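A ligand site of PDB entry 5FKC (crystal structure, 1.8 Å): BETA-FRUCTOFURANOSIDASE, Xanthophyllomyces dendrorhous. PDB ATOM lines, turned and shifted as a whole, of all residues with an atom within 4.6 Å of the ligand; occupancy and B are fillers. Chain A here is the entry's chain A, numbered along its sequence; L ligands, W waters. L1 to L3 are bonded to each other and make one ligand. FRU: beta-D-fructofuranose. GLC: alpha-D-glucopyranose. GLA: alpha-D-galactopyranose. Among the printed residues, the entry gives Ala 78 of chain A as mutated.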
ATOM      1  N   ASN A  77     -19.730   0.617 -15.886  1.00  0.00           N
ATOM      2  CA  ASN A  77     -18.655  -0.202 -15.359  1.00  0.00           C
ATOM      3  C   ASN A  77     -17.903   0.509 -14.224  1.00  0.00           C
ATOM      4  O   ASN A  77     -18.510   0.794 -13.193  1.00  0.00           O
ATOM      5  CB  ASN A  77     -17.787  -0.892 -16.454  1.00  0.00           C
ATOM      6  CG  ASN A  77     -17.132   0.063 -17.447  1.00  0.00           C
ATOM      7  OD1 ASN A  77     -17.792   0.746 -18.216  1.00  0.00           O
ATOM      8  ND2 ASN A  77     -15.802   0.040 -17.473  1.00  0.00           N
ATOM      9  N   ALA A  78     -16.613   0.797 -14.392  1.00  0.00           N
ATOM     10  CA  ALA A  78     -15.732   1.189 -13.286  1.00  0.00           C
ATOM     11  C   ALA A  78     -16.180   2.460 -12.577  1.00  0.00           C
ATOM     12  O   ALA A  78     -16.533   3.437 -13.230  1.00  0.00           O
ATOM     13  CB  ALA A  78     -14.318   1.397 -13.807  1.00  0.00           C
ATOM     14  N   GLN A  95     -18.021   4.941 -15.152  1.00  0.00           N
ATOM     15  CA  GLN A  95     -17.993   4.707 -16.580  1.00  0.00           C
ATOM     16  C   GLN A  95     -19.428   4.383 -17.012  1.00  0.00           C
ATOM     17  O   GLN A  95     -20.035   3.481 -16.431  1.00  0.00           O
ATOM     18  CB  GLN A  95     -17.046   3.546 -16.910  1.00  0.00           C
ATOM     19  CG  GLN A  95     -15.576   3.866 -16.632  1.00  0.00           C
ATOM     20  CD  GLN A  95     -14.953   4.703 -17.726  1.00  0.00           C
ATOM     21  OE1 GLN A  95     -14.501   4.179 -18.723  1.00  0.00           O
ATOM     22  NE2 GLN A  95     -14.941   6.030 -17.531  1.00  0.00           N
ATOM     23  N   TRP A 103     -20.666  -1.546 -23.682  1.00  0.00           N
ATOM     24  CA  TRP A 103     -19.752  -0.416 -23.541  1.00  0.00           C
ATOM     25  C   TRP A 103     -19.624   0.396 -24.826  1.00  0.00           C
ATOM     26  O   TRP A 103     -19.673  -0.142 -25.928  1.00  0.00           O
ATOM     27  CB  TRP A 103     -18.392  -0.994 -23.135  1.00  0.00           C
ATOM     28  CG  TRP A 103     -17.260  -0.063 -22.833  1.00  0.00           C
ATOM     29  CD1 TRP A 103     -16.825   0.309 -21.595  1.00  0.00           C
ATOM     30  CD2 TRP A 103     -16.360   0.538 -23.767  1.00  0.00           C
ATOM     31  NE1 TRP A 103     -15.721   1.116 -21.697  1.00  0.00           N
ATOM     32  CE2 TRP A 103     -15.408   1.278 -23.020  1.00  0.00           C
ATOM     33  CE3 TRP A 103     -16.252   0.514 -25.161  1.00  0.00           C
ATOM     34  CZ2 TRP A 103     -14.384   1.994 -23.619  1.00  0.00           C
ATOM     35  CZ3 TRP A 103     -15.227   1.229 -25.760  1.00  0.00           C
ATOM     36  CH2 TRP A 103     -14.296   1.952 -24.987  1.00  0.00           C
ATOM     37  N   ILE A 106     -17.642   6.053 -23.898  1.00  0.00           N
ATOM     38  CA  ILE A 106     -17.691   5.897 -22.460  1.00  0.00           C
ATOM     39  C   ILE A 106     -17.474   7.261 -21.796  1.00  0.00           C
ATOM     40  O   ILE A 106     -16.628   8.045 -22.206  1.00  0.00           O
ATOM     41  CB  ILE A 106     -16.770   4.768 -21.964  1.00  0.00           C
ATOM     42  CG1 ILE A 106     -17.287   4.201 -20.629  1.00  0.00           C
ATOM     43  CG2 ILE A 106     -15.315   5.221 -21.874  1.00  0.00           C
ATOM     44  CD1 ILE A 106     -18.551   3.362 -20.745  1.00  0.00           C
ATOM     45  N   ARG A 140     -12.678   8.715 -28.342  1.00  0.00           N
ATOM     46  CA  ARG A 140     -12.873   7.277 -28.289  1.00  0.00           C
ATOM     47  C   ARG A 140     -13.349   6.802 -26.916  1.00  0.00           C
ATOM     48  O   ARG A 140     -13.704   5.642 -26.763  1.00  0.00           O
ATOM     49  CB  ARG A 140     -11.583   6.569 -28.716  1.00  0.00           C
ATOM     50  CG  ARG A 140     -11.717   5.075 -28.975  1.00  0.00           C
ATOM     51  CD  ARG A 140     -11.123   4.214 -27.890  1.00  0.00           C
ATOM     52  NE  ARG A 140     -11.044   2.839 -28.347  1.00  0.00           N
ATOM     53  CZ  ARG A 140     -10.112   2.352 -29.168  1.00  0.00           C
ATOM     54  NH1 ARG A 140      -9.139   3.140 -29.653  1.00  0.00           N
ATOM     55  NH2 ARG A 140     -10.156   1.075 -29.528  1.00  0.00           N
ATOM     56  N   PHE A 143     -12.093   7.510 -20.216  1.00  0.00           N
ATOM     57  CA  PHE A 143     -11.815   6.334 -19.383  1.00  0.00           C
ATOM     58  C   PHE A 143     -11.676   6.768 -17.908  1.00  0.00           C
ATOM     59  O   PHE A 143     -11.955   7.928 -17.561  1.00  0.00           O
ATOM     60  CB  PHE A 143     -10.545   5.610 -19.876  1.00  0.00           C
ATOM     61  CG  PHE A 143     -10.742   4.696 -21.057  1.00  0.00           C
ATOM     62  CD1 PHE A 143     -11.652   4.970 -22.068  1.00  0.00           C
ATOM     63  CD2 PHE A 143      -9.934   3.571 -21.186  1.00  0.00           C
ATOM     64  CE1 PHE A 143     -11.767   4.141 -23.171  1.00  0.00           C
ATOM     65  CE2 PHE A 143     -10.051   2.725 -22.287  1.00  0.00           C
ATOM     66  CZ  PHE A 143     -10.985   3.010 -23.278  1.00  0.00           C
ATOM     67  N   ASP A 144     -11.300   5.834 -17.047  1.00  0.00           N
ATOM     68  CA  ASP A 144     -11.153   6.069 -15.605  1.00  0.00           C
ATOM     69  C   ASP A 144     -10.227   7.272 -15.319  1.00  0.00           C
ATOM     70  O   ASP A 144      -9.310   7.579 -16.076  1.00  0.00           O
ATOM     71  CB  ASP A 144     -10.609   4.778 -14.959  1.00  0.00           C
ATOM     72  CG  ASP A 144     -10.597   4.800 -13.435  1.00  0.00           C
ATOM     73  OD1 ASP A 144     -11.314   5.586 -12.779  1.00  0.00           O
ATOM     74  OD2 ASP A 144      -9.854   3.923 -12.886  1.00  0.00           O
ATOM     75  N   LEU A 168      -6.542  -0.797 -29.079  1.00  0.00           N
ATOM     76  CA  LEU A 168      -6.417  -0.492 -27.665  1.00  0.00           C
ATOM     77  C   LEU A 168      -6.659  -1.787 -26.904  1.00  0.00           C
ATOM     78  O   LEU A 168      -7.749  -2.375 -26.978  1.00  0.00           O
ATOM     79  CB  LEU A 168      -7.430   0.586 -27.263  1.00  0.00           C
ATOM     80  CG  LEU A 168      -7.247   1.271 -25.888  1.00  0.00           C
ATOM     81  CD1 LEU A 168      -8.124   2.517 -25.813  1.00  0.00           C
ATOM     82  CD2 LEU A 168      -7.536   0.331 -24.736  1.00  0.00           C
ATOM     83  N   GLY A 169      -5.642  -2.260 -26.187  1.00  0.00           N
ATOM     84  CA  GLY A 169      -5.782  -3.478 -25.399  1.00  0.00           C
ATOM     85  C   GLY A 169      -4.484  -4.181 -25.142  1.00  0.00           C
ATOM     86  O   GLY A 169      -3.539  -4.076 -25.948  1.00  0.00           O
ATOM     87  N   LEU A 172      -3.565  -6.552 -27.942  1.00  0.00           N
ATOM     88  CA  LEU A 172      -3.456  -5.933 -29.257  1.00  0.00           C
ATOM     89  C   LEU A 172      -2.142  -5.178 -29.354  1.00  0.00           C
ATOM     90  O   LEU A 172      -1.378  -5.121 -28.399  1.00  0.00           O
ATOM     91  CB  LEU A 172      -4.633  -4.986 -29.484  1.00  0.00           C
ATOM     92  CG  LEU A 172      -6.010  -5.638 -29.427  1.00  0.00           C
ATOM     93  CD1 LEU A 172      -7.101  -4.592 -29.615  1.00  0.00           C
ATOM     94  CD2 LEU A 172      -6.130  -6.736 -30.488  1.00  0.00           C
ATOM     95  N   ARG A 218      -3.142   3.660 -18.699  1.00  0.00           N
ATOM     96  CA  ARG A 218      -4.408   4.257 -18.291  1.00  0.00           C
ATOM     97  C   ARG A 218      -4.666   4.242 -16.795  1.00  0.00           C
ATOM     98  O   ARG A 218      -3.869   3.683 -16.010  1.00  0.00           O
ATOM     99  CB  ARG A 218      -5.568   3.585 -19.044  1.00  0.00           C
ATOM    100  CG  ARG A 218      -5.702   2.077 -18.849  1.00  0.00           C
ATOM    101  CD  ARG A 218      -7.049   1.577 -19.388  1.00  0.00           C
ATOM    102  NE  ARG A 218      -7.082   0.118 -19.484  1.00  0.00           N
ATOM    103  CZ  ARG A 218      -6.463  -0.610 -20.424  1.00  0.00           C
ATOM    104  NH1 ARG A 218      -5.768  -0.027 -21.402  1.00  0.00           N
ATOM    105  NH2 ARG A 218      -6.520  -1.939 -20.374  1.00  0.00           N
ATOM    106  N   ASP A 219      -5.774   4.872 -16.424  1.00  0.00           N
ATOM    107  CA  ASP A 219      -6.327   4.821 -15.080  1.00  0.00           C
ATOM    108  C   ASP A 219      -5.425   5.572 -14.093  1.00  0.00           C
ATOM    109  O   ASP A 219      -4.981   5.002 -13.097  1.00  0.00           O
ATOM    110  CB  ASP A 219      -6.604   3.377 -14.644  1.00  0.00           C
ATOM    111  CG  ASP A 219      -7.495   2.608 -15.631  1.00  0.00           C
ATOM    112  OD1 ASP A 219      -8.150   3.258 -16.476  1.00  0.00           O
ATOM    113  OD2 ASP A 219      -7.513   1.364 -15.558  1.00  0.00           O
ATOM    114  N   GLU A 301      -4.714  -2.671 -14.302  1.00  0.00           N
ATOM    115  CA  GLU A 301      -5.739  -1.647 -14.507  1.00  0.00           C
ATOM    116  C   GLU A 301      -6.187  -1.097 -13.160  1.00  0.00           C
ATOM    117  O   GLU A 301      -6.041  -1.763 -12.131  1.00  0.00           O
ATOM    118  CB  GLU A 301      -6.946  -2.234 -15.231  1.00  0.00           C
ATOM    119  CG  GLU A 301      -6.632  -2.833 -16.597  1.00  0.00           C
ATOM    120  CD  GLU A 301      -7.851  -3.438 -17.239  1.00  0.00           C
ATOM    121  OE1 GLU A 301      -8.468  -4.336 -16.631  1.00  0.00           O
ATOM    122  OE2 GLU A 301      -8.181  -3.038 -18.363  1.00  0.00           O
ATOM    123  N   THR A 302      -6.771   0.092 -13.193  1.00  0.00           N
ATOM    124  CA  THR A 302      -7.381   0.766 -12.042  1.00  0.00           C
ATOM    125  C   THR A 302      -6.580   0.643 -10.753  1.00  0.00           C
ATOM    126  O   THR A 302      -7.155   0.441  -9.692  1.00  0.00           O
ATOM    127  CB  THR A 302      -8.864   0.324 -11.801  1.00  0.00           C
ATOM    128  OG1 THR A 302      -8.912  -0.988 -11.223  1.00  0.00           O
ATOM    129  CG2 THR A 302      -9.660   0.340 -13.094  1.00  0.00           C
ATOM    130  N   GLU A 332      -5.187  -8.395 -15.799  1.00  0.00           N
ATOM    131  CA  GLU A 332      -5.835  -8.965 -16.964  1.00  0.00           C
ATOM    132  C   GLU A 332      -5.094 -10.191 -17.492  1.00  0.00           C
ATOM    133  O   GLU A 332      -3.869 -10.242 -17.469  1.00  0.00           O
ATOM    134  CB  GLU A 332      -5.868  -7.969 -18.111  1.00  0.00           C
ATOM    135  CG  GLU A 332      -6.392  -6.595 -17.776  1.00  0.00           C
ATOM    136  CD  GLU A 332      -6.794  -5.868 -19.043  1.00  0.00           C
ATOM    137  OE1 GLU A 332      -7.960  -6.050 -19.457  1.00  0.00           O
ATOM    138  OE2 GLU A 332      -5.944  -5.137 -19.611  1.00  0.00           O
ATOM    139  N   HIS A 341     -10.233 -11.324 -15.208  1.00  0.00           N
ATOM    140  CA  HIS A 341      -9.934 -10.185 -14.354  1.00  0.00           C
ATOM    141  C   HIS A 341      -9.821 -10.551 -12.874  1.00  0.00           C
ATOM    142  O   HIS A 341     -10.767 -11.104 -12.302  1.00  0.00           O
ATOM    143  CB  HIS A 341     -11.032  -9.127 -14.500  1.00  0.00           C
ATOM    144  CG  HIS A 341     -10.833  -8.185 -15.634  1.00  0.00           C
ATOM    145  ND1 HIS A 341     -11.883  -7.539 -16.262  1.00  0.00           N
ATOM    146  CD2 HIS A 341      -9.715  -7.768 -16.271  1.00  0.00           C
ATOM    147  CE1 HIS A 341     -11.422  -6.758 -17.216  1.00  0.00           C
ATOM    148  NE2 HIS A 341     -10.107  -6.874 -17.247  1.00  0.00           N
ATOM    149  N   TYR A 374     -14.681  -6.007 -10.007  1.00  0.00           N
ATOM    150  CA  TYR A 374     -13.442  -5.523 -10.578  1.00  0.00           C
ATOM    151  C   TYR A 374     -13.439  -4.007 -10.495  1.00  0.00           C
ATOM    152  O   TYR A 374     -14.470  -3.404 -10.167  1.00  0.00           O
ATOM    153  CB  TYR A 374     -13.333  -5.953 -12.044  1.00  0.00           C
ATOM    154  CG  TYR A 374     -11.960  -5.831 -12.658  1.00  0.00           C
ATOM    155  CD1 TYR A 374     -10.877  -6.540 -12.138  1.00  0.00           C
ATOM    156  CD2 TYR A 374     -11.742  -4.998 -13.752  1.00  0.00           C
ATOM    157  CE1 TYR A 374      -9.615  -6.439 -12.699  1.00  0.00           C
ATOM    158  CE2 TYR A 374     -10.486  -4.884 -14.318  1.00  0.00           C
ATOM    159  CZ  TYR A 374      -9.425  -5.606 -13.780  1.00  0.00           C
ATOM    160  OH  TYR A 374      -8.179  -5.515 -14.347  1.00  0.00           O
ATOM    161  N   TRP A 391     -16.962  -2.408  -9.028  1.00  0.00           N
ATOM    162  CA  TRP A 391     -18.060  -2.639  -9.960  1.00  0.00           C
ATOM    163  C   TRP A 391     -18.370  -4.121 -10.005  1.00  0.00           C
ATOM    164  O   TRP A 391     -17.450  -4.928 -10.143  1.00  0.00           O
ATOM    165  CB  TRP A 391     -17.652  -2.133 -11.333  1.00  0.00           C
ATOM    166  CG  TRP A 391     -18.268  -2.772 -12.550  1.00  0.00           C
ATOM    167  CD1 TRP A 391     -19.560  -2.717 -12.936  1.00  0.00           C
ATOM    168  CD2 TRP A 391     -17.557  -3.474 -13.574  1.00  0.00           C
ATOM    169  NE1 TRP A 391     -19.719  -3.363 -14.140  1.00  0.00           N
ATOM    170  CE2 TRP A 391     -18.501  -3.837 -14.555  1.00  0.00           C
ATOM    171  CE3 TRP A 391     -16.216  -3.840 -13.761  1.00  0.00           C
ATOM    172  CZ2 TRP A 391     -18.156  -4.551 -15.701  1.00  0.00           C
ATOM    173  CZ3 TRP A 391     -15.871  -4.553 -14.907  1.00  0.00           C
ATOM    174  CH2 TRP A 391     -16.831  -4.905 -15.858  1.00  0.00           C
HETATM  175  C1  FRU L   1     -11.244  -1.702 -16.441  1.00  0.00           C
HETATM  176  C2  FRU L   1     -11.238  -0.662 -17.565  1.00  0.00           C
HETATM  177  C3  FRU L   1     -10.298   0.481 -17.163  1.00  0.00           C
HETATM  178  C4  FRU L   1     -10.741   1.589 -18.117  1.00  0.00           C
HETATM  179  C5  FRU L   1     -12.259   1.369 -18.139  1.00  0.00           C
HETATM  180  C6  FRU L   1     -12.892   1.666 -19.500  1.00  0.00           C
HETATM  181  O1  FRU L   1     -12.094  -2.823 -16.697  1.00  0.00           O
HETATM  182  O2  FRU L   1     -10.822  -1.226 -18.814  1.00  0.00           O
HETATM  183  O3  FRU L   1      -8.922   0.115 -17.261  1.00  0.00           O
HETATM  184  O4  FRU L   1     -10.408   2.920 -17.664  1.00  0.00           O
HETATM  185  O5  FRU L   1     -12.479   0.012 -17.749  1.00  0.00           O
HETATM  186  O6  FRU L   1     -14.328   1.771 -19.398  1.00  0.00           O
HETATM  187  C1  GLC L   2     -11.722  -2.093 -19.521  1.00  0.00           C
HETATM  188  C2  GLC L   2     -11.066  -3.450 -19.808  1.00  0.00           C
HETATM  189  C3  GLC L   2      -9.931  -3.323 -20.820  1.00  0.00           C
HETATM  190  C4  GLC L   2     -10.476  -2.681 -22.081  1.00  0.00           C
HETATM  191  C5  GLC L   2     -11.157  -1.339 -21.756  1.00  0.00           C
HETATM  192  C6  GLC L   2     -11.879  -0.799 -22.983  1.00  0.00           C
HETATM  193  O2  GLC L   2     -10.602  -4.056 -18.591  1.00  0.00           O
HETATM  194  O3  GLC L   2      -9.387  -4.622 -21.090  1.00  0.00           O
HETATM  195  O4  GLC L   2      -9.438  -2.445 -23.025  1.00  0.00           O
HETATM  196  O5  GLC L   2     -12.132  -1.480 -20.726  1.00  0.00           O
HETATM  197  O6  GLC L   2     -12.722  -1.847 -23.463  1.00  0.00           O
HETATM  198  C1  GLA L   3     -13.503  -1.547 -24.605  1.00  0.00           C
HETATM  199  C2  GLA L   3     -14.502  -2.668 -24.887  1.00  0.00           C
HETATM  200  C3  GLA L   3     -13.756  -3.950 -25.228  1.00  0.00           C
HETATM  201  C4  GLA L   3     -12.802  -3.706 -26.405  1.00  0.00           C
HETATM  202  C5  GLA L   3     -11.897  -2.489 -26.120  1.00  0.00           C
HETATM  203  C6  GLA L   3     -11.027  -2.045 -27.293  1.00  0.00           C
HETATM  204  O2  GLA L   3     -15.332  -2.863 -23.747  1.00  0.00           O
HETATM  205  O3  GLA L   3     -14.722  -4.984 -25.519  1.00  0.00           O
HETATM  206  O4  GLA L   3     -13.580  -3.524 -27.603  1.00  0.00           O
HETATM  207  O5  GLA L   3     -12.685  -1.338 -25.736  1.00  0.00           O
HETATM  208  O6  GLA L   3     -10.118  -3.093 -27.603  1.00  0.00           O
HETATM  209  O   HOH W   1     -12.926  -3.356 -30.144  1.00  0.00           O
HETATM  210  O   HOH W   2     -10.750  -5.673 -28.846  1.00  0.00           O
HETATM  211  O   HOH W   3      -8.988  -4.418 -24.714  1.00  0.00           O
HETATM  212  O   HOH W   4      -9.061  -1.858 -30.226  1.00  0.00           O
HETATM  213  O   HOH W   5      -6.612  -4.446 -22.152  1.00  0.00           O
HETATM  214  O   HOH W   6     -11.194  -6.271 -22.191  1.00  0.00           O
HETATM  215  O   HOH W   7     -14.495  -2.035 -15.994  1.00  0.00           O
HETATM  216  O   HOH W   8     -17.058  -4.872 -23.396  1.00  0.00           O
HETATM  217  O   HOH W   9     -15.777  -2.013 -28.219  1.00  0.00           O
HETATM  218  O   HOH W  10     -12.871   0.567 -28.015  1.00  0.00           O
HETATM  219  O   HOH W  11     -14.600  -2.911 -21.142  1.00  0.00           O
HETATM  220  O   HOH W  12     -15.113  -5.656 -28.605  1.00  0.00           O
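OE1 of Gln 95 lies within hydrogen-bond range of O6 of FRU L1. O3 of FRU L1 lies within hydrogen-bond range of OD2 of Asp 219. The backbone carbonyl oxygen of Leu 168 sits at hydrogen-bond distance from an oxygen (O6) of GLA L3 (2.6 Å). OE1 of Glu 332 sits at hydrogen-bond distance from O3 of GLC L2, at 2.6 Å. O2 of GLC L2 sits at hydrogen-bond distance from OE2 of Glu 301 (2.6 Å). NE1 of Trp 103 is in hydrogen-bond range of O6 of FRU L1, 2.8 Å away. The guanidinium group of Arg 218 is in hydrogen-bond range of an oxygen (O3) of FRU L1. An oxygen (O6) of FRU L1 sits at hydrogen-bond distance from the side-chain amide nitrogen (ND2) of Asn 77 (3.0 Å). O4 of FRU L1 is in hydrogen-bond range of N of Asp 144 (3.1 Å). An oxygen (O2) of GLC L2 sits close to a ring nitrogen (NE2) of His 341.
The backbone carbonyl oxygen of Ala 78 sits at hydrogen-bond distance from the backbone NH of Gln 95 (2.9 Å). The side-chain carboxylate (OD2) of Asp 219 lies within hydrogen-bond range of the backbone NH (N) of Thr 302. The side-chain carboxylate (OE2) of Glu 332 is in salt-bridge range of the guanidinium group (NH2) of Arg 218 (3.3 Å). The side-chain carboxylate (OE1) of Glu 332 lies within hydrogen-bond range of a ring nitrogen (NE2) of His 341. NH2 of Arg 218 lies within salt-bridge range of OE2 of Glu 301 (2.8 Å). A ring nitrogen (NE2) of His 341 is in hydrogen-bond range of the side-chain carboxylate (OE1) of Glu 301. The side-chain carboxylate (OE1) of Glu 301 lies within hydrogen-bond range of the side-chain hydroxyl (OH) of Tyr 374. The backbone carbonyl oxygen (O) of Tyr 374 lies within hydrogen-bond range of the backbone NH (N) of Trp 391 (2.9 Å).
Residues that only touch the ligand: Phe 143, Tyr 374, Leu 172 and Arg 140. Hydrophobic or aromatic side chains that line the ligand: Trp 103, Phe 143, Leu 168, Leu 172, His 341 and Tyr 374. Of the 19 residues printed, 14 come within 4 Å of the ligand. The nearest printed residue that does not touch the ligand is Ile 106 (4.02 Å).
Water W7 lies within hydrogen-bond range of O1 of FRU L1 (2.6 Å) and ND2 of Asn 77 (2.9 Å). Water W3 bridges an oxygen (O4) of GLC L2 (2.6 Å) and the backbone carbonyl oxygen (O) of Leu 168 (3.3 Å). Water W10 lies within hydrogen-bond range of the guanidinium group (NE) of Arg 140 (2.9 Å) and an oxygen (O5) of GLA L3 (3.0 Å). Water W5 lies within hydrogen-bond range of OE2 of Glu 332 (2.7 Å), O3 of GLC L2 (3.0 Å) and NH2 of Arg 218 (3.1 Å). Water W4 lies within hydrogen-bond range of N of Leu 168 (3.0 Å), O6 of GLA L3 (3.1 Å) and NH2 of Arg 140 (3.2 Å).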
